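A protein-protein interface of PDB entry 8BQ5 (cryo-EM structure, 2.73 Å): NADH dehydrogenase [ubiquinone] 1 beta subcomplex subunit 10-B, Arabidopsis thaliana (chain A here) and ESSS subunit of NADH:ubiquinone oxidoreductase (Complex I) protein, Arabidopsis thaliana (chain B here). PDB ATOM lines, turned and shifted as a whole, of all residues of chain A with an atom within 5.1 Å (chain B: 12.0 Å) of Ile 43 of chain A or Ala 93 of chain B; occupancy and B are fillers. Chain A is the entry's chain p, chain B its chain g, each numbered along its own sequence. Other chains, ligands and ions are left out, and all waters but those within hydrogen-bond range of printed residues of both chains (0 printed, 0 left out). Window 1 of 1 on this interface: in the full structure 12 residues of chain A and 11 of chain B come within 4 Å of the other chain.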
ATOM      1  N   ARG A  39      25.094  12.151  -7.173  1.00  0.00           N
ATOM      2  CA  ARG A  39      25.210  12.882  -8.430  1.00  0.00           C
ATOM      3  C   ARG A  39      24.319  14.116  -8.432  1.00  0.00           C
ATOM      4  O   ARG A  39      24.705  15.169  -8.954  1.00  0.00           O
ATOM      5  CB  ARG A  39      24.863  11.964  -9.600  1.00  0.00           C
ATOM      6  CG  ARG A  39      26.056  11.558 -10.452  1.00  0.00           C
ATOM      7  CD  ARG A  39      26.125  10.056 -10.628  1.00  0.00           C
ATOM      8  NE  ARG A  39      24.827   9.479 -10.947  1.00  0.00           N
ATOM      9  CZ  ARG A  39      24.557   8.183 -10.900  1.00  0.00           C
ATOM     10  NH1 ARG A  39      25.478   7.298 -10.560  1.00  0.00           N
ATOM     11  NH2 ARG A  39      23.331   7.763 -11.199  1.00  0.00           N
ATOM     12  N   GLU A  40      23.118  14.005  -7.860  1.00  0.00           N
ATOM     13  CA  GLU A  40      22.225  15.155  -7.785  1.00  0.00           C
ATOM     14  C   GLU A  40      22.824  16.250  -6.913  1.00  0.00           C
ATOM     15  O   GLU A  40      22.755  17.435  -7.254  1.00  0.00           O
ATOM     16  CB  GLU A  40      20.849  14.737  -7.254  1.00  0.00           C
ATOM     17  CG  GLU A  40      19.893  14.001  -8.234  1.00  0.00           C
ATOM     18  CD  GLU A  40      19.652  14.705  -9.575  1.00  0.00           C
ATOM     19  OE1 GLU A  40      20.545  15.413 -10.079  1.00  0.00           O
ATOM     20  OE2 GLU A  40      18.552  14.551 -10.141  1.00  0.00           O
ATOM     21  N   LYS A  41      23.416  15.870  -5.779  1.00  0.00           N
ATOM     22  CA  LYS A  41      24.012  16.862  -4.891  1.00  0.00           C
ATOM     23  C   LYS A  41      25.202  17.546  -5.546  1.00  0.00           C
ATOM     24  O   LYS A  41      25.449  18.735  -5.313  1.00  0.00           O
ATOM     25  CB  LYS A  41      24.425  16.210  -3.573  1.00  0.00           C
ATOM     26  CG  LYS A  41      23.272  15.959  -2.619  1.00  0.00           C
ATOM     27  CD  LYS A  41      23.772  15.421  -1.292  1.00  0.00           C
ATOM     28  CE  LYS A  41      22.656  15.319  -0.273  1.00  0.00           C
ATOM     29  NZ  LYS A  41      23.183  15.336   1.118  1.00  0.00           N
ATOM     30  N   TRP A  42      25.955  16.814  -6.368  1.00  0.00           N
ATOM     31  CA  TRP A  42      27.101  17.416  -7.037  1.00  0.00           C
ATOM     32  C   TRP A  42      26.654  18.428  -8.081  1.00  0.00           C
ATOM     33  O   TRP A  42      27.346  19.421  -8.327  1.00  0.00           O
ATOM     34  CB  TRP A  42      27.973  16.331  -7.664  1.00  0.00           C
ATOM     35  CG  TRP A  42      29.013  15.813  -6.725  1.00  0.00           C
ATOM     36  CD1 TRP A  42      29.013  14.607  -6.088  1.00  0.00           C
ATOM     37  CD2 TRP A  42      30.193  16.496  -6.291  1.00  0.00           C
ATOM     38  NE1 TRP A  42      30.128  14.492  -5.295  1.00  0.00           N
ATOM     39  CE2 TRP A  42      30.869  15.639  -5.402  1.00  0.00           C
ATOM     40  CE3 TRP A  42      30.748  17.749  -6.573  1.00  0.00           C
ATOM     41  CZ2 TRP A  42      32.070  15.992  -4.792  1.00  0.00           C
ATOM     42  CZ3 TRP A  42      31.940  18.098  -5.967  1.00  0.00           C
ATOM     43  CH2 TRP A  42      32.589  17.222  -5.087  1.00  0.00           C
ATOM     44  N   ILE A  43      25.497  18.194  -8.702  1.00  0.00           N
ATOM     45  CA  ILE A  43      24.937  19.173  -9.627  1.00  0.00           C
ATOM     46  C   ILE A  43      24.582  20.460  -8.889  1.00  0.00           C
ATOM     47  O   ILE A  43      24.842  21.564  -9.382  1.00  0.00           O
ATOM     48  CB  ILE A  43      23.724  18.575 -10.365  1.00  0.00           C
ATOM     49  CG1 ILE A  43      24.175  17.440 -11.286  1.00  0.00           C
ATOM     50  CG2 ILE A  43      22.996  19.639 -11.166  1.00  0.00           C
ATOM     51  CD1 ILE A  43      23.074  16.478 -11.653  1.00  0.00           C
ATOM     52  N   GLN A  44      23.991  20.342  -7.695  1.00  0.00           N
ATOM     53  CA  GLN A  44      23.689  21.533  -6.904  1.00  0.00           C
ATOM     54  C   GLN A  44      24.958  22.267  -6.493  1.00  0.00           C
ATOM     55  O   GLN A  44      24.996  23.503  -6.501  1.00  0.00           O
ATOM     56  CB  GLN A  44      22.870  21.174  -5.663  1.00  0.00           C
ATOM     57  CG  GLN A  44      21.967  19.973  -5.813  1.00  0.00           C
ATOM     58  CD  GLN A  44      20.663  20.306  -6.508  1.00  0.00           C
ATOM     59  OE1 GLN A  44      20.640  21.052  -7.487  1.00  0.00           O
ATOM     60  NE2 GLN A  44      19.569  19.747  -6.010  1.00  0.00           N
ATOM     61  N   ILE A  45      26.001  21.528  -6.106  1.00  0.00           N
ATOM     62  CA  ILE A  45      27.253  22.170  -5.712  1.00  0.00           C
ATOM     63  C   ILE A  45      27.829  22.959  -6.879  1.00  0.00           C
ATOM     64  O   ILE A  45      28.275  24.101  -6.721  1.00  0.00           O
ATOM     65  CB  ILE A  45      28.263  21.136  -5.187  1.00  0.00           C
ATOM     66  CG1 ILE A  45      27.760  20.475  -3.906  1.00  0.00           C
ATOM     67  CG2 ILE A  45      29.610  21.788  -4.935  1.00  0.00           C
ATOM     68  CD1 ILE A  45      28.200  19.047  -3.774  1.00  0.00           C
ATOM     69  N   GLU A  46      27.826  22.362  -8.071  1.00  0.00           N
ATOM     70  CA  GLU A  46      28.348  23.064  -9.235  1.00  0.00           C
ATOM     71  C   GLU A  46      27.387  24.150  -9.701  1.00  0.00           C
ATOM     72  O   GLU A  46      27.810  25.122 -10.335  1.00  0.00           O
ATOM     73  CB  GLU A  46      28.635  22.072 -10.360  1.00  0.00           C
ATOM     74  CG  GLU A  46      29.547  20.929  -9.943  1.00  0.00           C
ATOM     75  CD  GLU A  46      31.015  21.248 -10.119  1.00  0.00           C
ATOM     76  OE1 GLU A  46      31.646  21.720  -9.151  1.00  0.00           O
ATOM     77  OE2 GLU A  46      31.543  21.035 -11.226  1.00  0.00           O
ATOM     78  N   LYS A  47      26.096  23.999  -9.398  1.00  0.00           N
ATOM     79  CA  LYS A  47      25.135  25.072  -9.638  1.00  0.00           C
ATOM     80  C   LYS A  47      25.509  26.321  -8.853  1.00  0.00           C
ATOM     81  O   LYS A  47      25.571  27.424  -9.408  1.00  0.00           O
ATOM     82  CB  LYS A  47      23.732  24.607  -9.249  1.00  0.00           C
ATOM     83  CG  LYS A  47      22.614  25.074 -10.161  1.00  0.00           C
ATOM     84  CD  LYS A  47      22.660  24.362 -11.498  1.00  0.00           C
ATOM     85  CE  LYS A  47      21.273  24.267 -12.114  1.00  0.00           C
ATOM     86  NZ  LYS A  47      20.540  23.054 -11.656  1.00  0.00           N
ATOM     87  N   ALA A  48      25.760  26.162  -7.552  1.00  0.00           N
ATOM     88  CA  ALA A  48      26.158  27.291  -6.720  1.00  0.00           C
ATOM     89  C   ALA A  48      27.520  27.836  -7.123  1.00  0.00           C
ATOM     90  O   ALA A  48      27.750  29.047  -7.049  1.00  0.00           O
ATOM     91  CB  ALA A  48      26.166  26.878  -5.250  1.00  0.00           C
ATOM     92  N   ASP B  86      39.043  12.768 -18.511  1.00  0.00           N
ATOM     93  CA  ASP B  86      38.597  13.482 -17.321  1.00  0.00           C
ATOM     94  C   ASP B  86      37.218  12.973 -16.933  1.00  0.00           C
ATOM     95  O   ASP B  86      36.198  13.519 -17.365  1.00  0.00           O
ATOM     96  CB  ASP B  86      38.580  14.988 -17.562  1.00  0.00           C
ATOM     97  CG  ASP B  86      38.697  15.778 -16.275  1.00  0.00           C
ATOM     98  OD1 ASP B  86      37.809  15.638 -15.409  1.00  0.00           O
ATOM     99  OD2 ASP B  86      39.684  16.525 -16.125  1.00  0.00           O
ATOM    100  N   LEU B  87      37.185  11.924 -16.113  1.00  0.00           N
ATOM    101  CA  LEU B  87      35.943  11.304 -15.676  1.00  0.00           C
ATOM    102  C   LEU B  87      35.563  11.713 -14.260  1.00  0.00           C
ATOM    103  O   LEU B  87      34.702  11.078 -13.647  1.00  0.00           O
ATOM    104  CB  LEU B  87      36.049   9.783 -15.784  1.00  0.00           C
ATOM    105  CG  LEU B  87      36.586   9.285 -17.126  1.00  0.00           C
ATOM    106  CD1 LEU B  87      36.849   7.788 -17.089  1.00  0.00           C
ATOM    107  CD2 LEU B  87      35.630   9.642 -18.255  1.00  0.00           C
ATOM    108  N   SER B  88      36.186  12.761 -13.728  1.00  0.00           N
ATOM    109  CA  SER B  88      35.867  13.208 -12.380  1.00  0.00           C
ATOM    110  C   SER B  88      34.410  13.651 -12.295  1.00  0.00           C
ATOM    111  O   SER B  88      33.836  14.169 -13.258  1.00  0.00           O
ATOM    112  CB  SER B  88      36.793  14.349 -11.965  1.00  0.00           C
ATOM    113  OG  SER B  88      36.496  15.532 -12.685  1.00  0.00           O
ATOM    114  N   ILE B  89      33.807  13.426 -11.124  1.00  0.00           N
ATOM    115  CA  ILE B  89      32.397  13.760 -10.929  1.00  0.00           C
ATOM    116  C   ILE B  89      32.162  15.250 -11.123  1.00  0.00           C
ATOM    117  O   ILE B  89      31.135  15.657 -11.680  1.00  0.00           O
ATOM    118  CB  ILE B  89      31.921  13.287  -9.539  1.00  0.00           C
ATOM    119  CG1 ILE B  89      30.529  13.836  -9.227  1.00  0.00           C
ATOM    120  CG2 ILE B  89      32.911  13.697  -8.457  1.00  0.00           C
ATOM    121  CD1 ILE B  89      29.416  13.139  -9.965  1.00  0.00           C
ATOM    122  N   GLU B  90      33.109  16.082 -10.688  1.00  0.00           N
ATOM    123  CA  GLU B  90      32.946  17.527 -10.805  1.00  0.00           C
ATOM    124  C   GLU B  90      32.806  17.952 -12.262  1.00  0.00           C
ATOM    125  O   GLU B  90      31.958  18.785 -12.598  1.00  0.00           O
ATOM    126  CB  GLU B  90      34.127  18.235 -10.141  1.00  0.00           C
ATOM    127  CG  GLU B  90      34.356  17.826  -8.691  1.00  0.00           C
ATOM    128  CD  GLU B  90      35.552  16.906  -8.508  1.00  0.00           C
ATOM    129  OE1 GLU B  90      36.179  16.954  -7.430  1.00  0.00           O
ATOM    130  OE2 GLU B  90      35.866  16.132  -9.436  1.00  0.00           O
ATOM    131  N   THR B  91      33.623  17.381 -13.149  1.00  0.00           N
ATOM    132  CA  THR B  91      33.531  17.737 -14.562  1.00  0.00           C
ATOM    133  C   THR B  91      32.173  17.354 -15.141  1.00  0.00           C
ATOM    134  O   THR B  91      31.592  18.110 -15.928  1.00  0.00           O
ATOM    135  CB  THR B  91      34.657  17.066 -15.348  1.00  0.00           C
ATOM    136  OG1 THR B  91      35.920  17.443 -14.789  1.00  0.00           O
ATOM    137  CG2 THR B  91      34.614  17.492 -16.806  1.00  0.00           C
ATOM    138  N   TRP B  92      31.658  16.179 -14.770  1.00  0.00           N
ATOM    139  CA  TRP B  92      30.350  15.754 -15.261  1.00  0.00           C
ATOM    140  C   TRP B  92      29.236  16.653 -14.737  1.00  0.00           C
ATOM    141  O   TRP B  92      28.337  17.040 -15.493  1.00  0.00           O
ATOM    142  CB  TRP B  92      30.091  14.299 -14.868  1.00  0.00           C
ATOM    143  CG  TRP B  92      28.687  13.842 -15.137  1.00  0.00           C
ATOM    144  CD1 TRP B  92      28.227  13.242 -16.269  1.00  0.00           C
ATOM    145  CD2 TRP B  92      27.565  13.938 -14.250  1.00  0.00           C
ATOM    146  NE1 TRP B  92      26.886  12.966 -16.149  1.00  0.00           N
ATOM    147  CE2 TRP B  92      26.457  13.382 -14.917  1.00  0.00           C
ATOM    148  CE3 TRP B  92      27.390  14.442 -12.958  1.00  0.00           C
ATOM    149  CZ2 TRP B  92      25.194  13.316 -14.336  1.00  0.00           C
ATOM    150  CZ3 TRP B  92      26.134  14.380 -12.386  1.00  0.00           C
ATOM    151  CH2 TRP B  92      25.053  13.818 -13.073  1.00  0.00           C
ATOM    152  N   ALA B  93      29.275  16.992 -13.447  1.00  0.00           N
ATOM    153  CA  ALA B  93      28.203  17.788 -12.858  1.00  0.00           C
ATOM    154  C   ALA B  93      28.238  19.230 -13.339  1.00  0.00           C
ATOM    155  O   ALA B  93      27.190  19.883 -13.404  1.00  0.00           O
ATOM    156  CB  ALA B  93      28.282  17.738 -11.334  1.00  0.00           C
ATOM    157  N   HIS B  94      29.420  19.750 -13.664  1.00  0.00           N
ATOM    158  CA  HIS B  94      29.508  21.113 -14.178  1.00  0.00           C
ATOM    159  C   HIS B  94      28.799  21.236 -15.520  1.00  0.00           C
ATOM    160  O   HIS B  94      28.092  22.217 -15.776  1.00  0.00           O
ATOM    161  CB  HIS B  94      30.968  21.538 -14.296  1.00  0.00           C
ATOM    162  CG  HIS B  94      31.145  22.944 -14.772  1.00  0.00           C
ATOM    163  ND1 HIS B  94      31.205  24.018 -13.910  1.00  0.00           N
ATOM    164  CD2 HIS B  94      31.272  23.453 -16.019  1.00  0.00           C
ATOM    165  CE1 HIS B  94      31.362  25.128 -14.608  1.00  0.00           C
ATOM    166  NE2 HIS B  94      31.406  24.814 -15.889  1.00  0.00           N
ATOM    167  N   GLN B  95      28.989  20.250 -16.399  1.00  0.00           N
ATOM    168  CA  GLN B  95      28.259  20.243 -17.661  1.00  0.00           C
ATOM    169  C   GLN B  95      26.764  20.081 -17.429  1.00  0.00           C
ATOM    170  O   GLN B  95      25.952  20.746 -18.083  1.00  0.00           O
ATOM    171  CB  GLN B  95      28.786  19.131 -18.568  1.00  0.00           C
ATOM    172  CG  GLN B  95      28.941  19.533 -20.026  1.00  0.00           C
ATOM    173  CD  GLN B  95      30.101  20.483 -20.262  1.00  0.00           C
ATOM    174  OE1 GLN B  95      30.745  20.949 -19.322  1.00  0.00           O
ATOM    175  NE2 GLN B  95      30.378  20.769 -21.529  1.00  0.00           N
ATOM    176  N   LYS B  96      26.382  19.205 -16.499  1.00  0.00           N
ATOM    177  CA  LYS B  96      24.967  19.001 -16.208  1.00  0.00           C
ATOM    178  C   LYS B  96      24.347  20.241 -15.573  1.00  0.00           C
ATOM    179  O   LYS B  96      23.165  20.526 -15.783  1.00  0.00           O
ATOM    180  CB  LYS B  96      24.795  17.787 -15.298  1.00  0.00           C
ATOM    181  CG  LYS B  96      24.855  16.450 -16.020  1.00  0.00           C
ATOM    182  CD  LYS B  96      23.530  16.097 -16.674  1.00  0.00           C
ATOM    183  CE  LYS B  96      23.701  14.999 -17.711  1.00  0.00           C
ATOM    184  NZ  LYS B  96      24.947  15.163 -18.506  1.00  0.00           N
ATOM    185  N   ALA B  97      25.127  20.983 -14.784  1.00  0.00           N
ATOM    186  CA  ALA B  97      24.608  22.194 -14.155  1.00  0.00           C
ATOM    187  C   ALA B  97      24.407  23.304 -15.178  1.00  0.00           C
ATOM    188  O   ALA B  97      23.490  24.123 -15.047  1.00  0.00           O
ATOM    189  CB  ALA B  97      25.548  22.656 -13.042  1.00  0.00           C
ATOM    190  N   LEU B  98      25.269  23.359 -16.195  1.00  0.00           N
ATOM    191  CA  LEU B  98      25.130  24.378 -17.228  1.00  0.00           C
ATOM    192  C   LEU B  98      23.855  24.183 -18.035  1.00  0.00           C
ATOM    193  O   LEU B  98      23.155  25.150 -18.357  1.00  0.00           O
ATOM    194  CB  LEU B  98      26.351  24.372 -18.146  1.00  0.00           C
ATOM    195  CG  LEU B  98      27.556  25.112 -17.575  1.00  0.00           C
ATOM    196  CD1 LEU B  98      28.787  24.875 -18.428  1.00  0.00           C
ATOM    197  CD2 LEU B  98      27.242  26.591 -17.462  1.00  0.00           C
ATOM    198  N   GLU B  99      23.539  22.934 -18.384  1.00  0.00           N
ATOM    199  CA  GLU B  99      22.362  22.701 -19.210  1.00  0.00           C
ATOM    200  C   GLU B  99      21.073  22.847 -18.407  1.00  0.00           C
ATOM    201  O   GLU B  99      20.097  23.408 -18.912  1.00  0.00           O
ATOM    202  CB  GLU B  99      22.455  21.333 -19.895  1.00  0.00           C
ATOM    203  CG  GLU B  99      21.974  20.143 -19.085  1.00  0.00           C
ATOM    204  CD  GLU B  99      22.637  18.843 -19.500  1.00  0.00           C
ATOM    205  OE1 GLU B  99      23.615  18.888 -20.277  1.00  0.00           O
ATOM    206  OE2 GLU B  99      22.170  17.773 -19.059  1.00  0.00           O
ATOM    207  N   ARG B 100      21.052  22.389 -17.152  1.00  0.00           N
ATOM    208  CA  ARG B 100      19.851  22.565 -16.343  1.00  0.00           C
ATOM    209  C   ARG B 100      19.595  24.039 -16.045  1.00  0.00           C
ATOM    210  O   ARG B 100      18.440  24.472 -15.986  1.00  0.00           O
ATOM    211  CB  ARG B 100      19.955  21.765 -15.046  1.00  0.00           C
ATOM    212  CG  ARG B 100      19.427  20.340 -15.154  1.00  0.00           C
ATOM    213  CD  ARG B 100      19.363  19.685 -13.788  1.00  0.00           C
ATOM    214  NE  ARG B 100      19.627  18.253 -13.835  1.00  0.00           N
ATOM    215  CZ  ARG B 100      19.587  17.454 -12.777  1.00  0.00           C
ATOM    216  NH1 ARG B 100      19.279  17.915 -11.577  1.00  0.00           N
ATOM    217  NH2 ARG B 100      19.871  16.163 -12.927  1.00  0.00           N
ATOM    218  N   LEU B 101      20.659  24.820 -15.846  1.00  0.00           N
ATOM    219  CA  LEU B 101      20.496  26.266 -15.753  1.00  0.00           C
ATOM    220  C   LEU B 101      20.067  26.866 -17.084  1.00  0.00           C
ATOM    221  O   LEU B 101      19.364  27.883 -17.106  1.00  0.00           O
ATOM    222  CB  LEU B 101      21.793  26.917 -15.272  1.00  0.00           C
ATOM    223  CG  LEU B 101      21.646  28.110 -14.327  1.00  0.00           C
ATOM    224  CD1 LEU B 101      20.936  27.708 -13.050  1.00  0.00           C
ATOM    225  CD2 LEU B 101      22.999  28.723 -14.015  1.00  0.00           C
ATOM    226  N   GLU B 102      20.488  26.266 -18.199  1.00  0.00           N
ATOM    227  CA  GLU B 102      20.052  26.742 -19.507  1.00  0.00           C
ATOM    228  C   GLU B 102      18.584  26.407 -19.749  1.00  0.00           C
ATOM    229  O   GLU B 102      17.805  27.264 -20.183  1.00  0.00           O
ATOM    230  CB  GLU B 102      20.927  26.134 -20.604  1.00  0.00           C
ATOM    231  CG  GLU B 102      22.092  27.006 -21.044  1.00  0.00           C
ATOM    232  CD  GLU B 102      21.657  28.364 -21.548  1.00  0.00           C
ATOM    233  OE1 GLU B 102      21.104  28.436 -22.664  1.00  0.00           O
ATOM    234  OE2 GLU B 102      21.883  29.362 -20.832  1.00  0.00           O
ATOM    235  N   MET B 103      18.186  25.163 -19.463  1.00  0.00           N
ATOM    236  CA  MET B 103      16.815  24.742 -19.735  1.00  0.00           C
ATOM    237  C   MET B 103      15.807  25.482 -18.865  1.00  0.00           C
ATOM    238  O   MET B 103      14.683  25.739 -19.309  1.00  0.00           O
ATOM    239  CB  MET B 103      16.674  23.229 -19.548  1.00  0.00           C
ATOM    240  CG  MET B 103      17.458  22.374 -20.552  1.00  0.00           C
ATOM    241  SD  MET B 103      17.031  22.602 -22.293  1.00  0.00           S
ATOM    242  CE  MET B 103      15.363  21.952 -22.341  1.00  0.00           C
ATOM    243  N   GLU B 104      16.175  25.826 -17.632  1.00  0.00           N
ATOM    244  CA  GLU B 104      15.259  26.543 -16.753  1.00  0.00           C
ATOM    245  C   GLU B 104      15.301  28.055 -16.941  1.00  0.00           C
ATOM    246  O   GLU B 104      14.426  28.753 -16.416  1.00  0.00           O
ATOM    247  CB  GLU B 104      15.548  26.207 -15.286  1.00  0.00           C
ATOM    248  CG  GLU B 104      16.385  27.245 -14.554  1.00  0.00           C
ATOM    249  CD  GLU B 104      16.450  26.986 -13.064  1.00  0.00           C
ATOM    250  OE1 GLU B 104      15.392  26.687 -12.469  1.00  0.00           O
ATOM    251  OE2 GLU B 104      17.554  27.078 -12.489  1.00  0.00           O
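Of the printed residues of chain B, Arg 39 of chain A touches Ile 89 and Trp 92.
Glu 40 of chain A touches just one residue of chain B: Arg 100 (3.0 Å).
Of chain B, only Ile 89, Glu 90 and Ala 93 come within 4 Å of Trp 42 of chain A.
No residue of chain B comes within 4 Å of Gln 44 of chain A.
No residue of chain B comes within 4 Å of Ile 45 of chain A.
Of chain A, only Trp 42 (3.6 Å), Ile 43 (3.9 Å) and Glu 46 (3.7 Å) come within 4 Å of Ala 93 of chain B.
Gln 95 of chain B touches none of the printed residues of chain A.
Leu 98 of chain B touches none of the printed residues of chain A.
Of the printed residues of chain A, Leu 101 of chain B touches Lys 47 (3.6 Å).
The nearest residue of chain A that does not touch Ala 93 of chain B is Arg 39 of chain A (5.0 Å).
Among the printed residues, merely in contact across the chains: Arg 39 of chain A with Ile 89 of chain B, Arg 39 of chain A with Trp 92 of chain B, Trp 42 of chain A with Ile 89 of chain B, Trp 42 of chain A with Glu 90 of chain B, Trp 42 of chain A with Ala 93 of chain B, Ile 43 of chain A with Trp 92 of chain B, Ile 43 of chain A with Ala 93 of chain B, Ile 43 of chain A with Ala 97 of chain B, Ile 43 of chain A with Arg 100 of chain B, Glu 46 of chain A with Ala 93 of chain B, Lys 47 of chain A with Ala 97 of chain B, Lys 47 of chain A with Arg 100 of chain B and Lys 47 of chain A with Leu 101 of chain B.
Of the 10 printed residues of chain A, 6 touch a printed residue of chain B.
Printed residues of chain A that touch a printed residue of chain B: Arg 39, Glu 40, Trp 42, Ile 43, Glu 46 and Lys 47.
Among the printed residues, Asp or Glu carboxylates within 4 Å of a Lys or Arg side-chain nitrogen of the other chain: Glu 40 of chain A with Arg 100 of chain B (3.0 Å).
OG of Ser 88 of chain B sits close to OE2 of Glu 90 of chain B (3.4 Å).
The backbone carbonyl oxygen (O) of Glu 90 of chain B sits close to the side-chain carboxylate (OE2) of Glu 46 of chain A (2.7 Å).
N of His 94 of chain B lies close to OE2 of Glu 46 of chain A (3.5 Å).
NH2 of Arg 100 of chain B is in salt-bridge range of OE1 of Glu 40 of chain A, at 3.0 Å.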
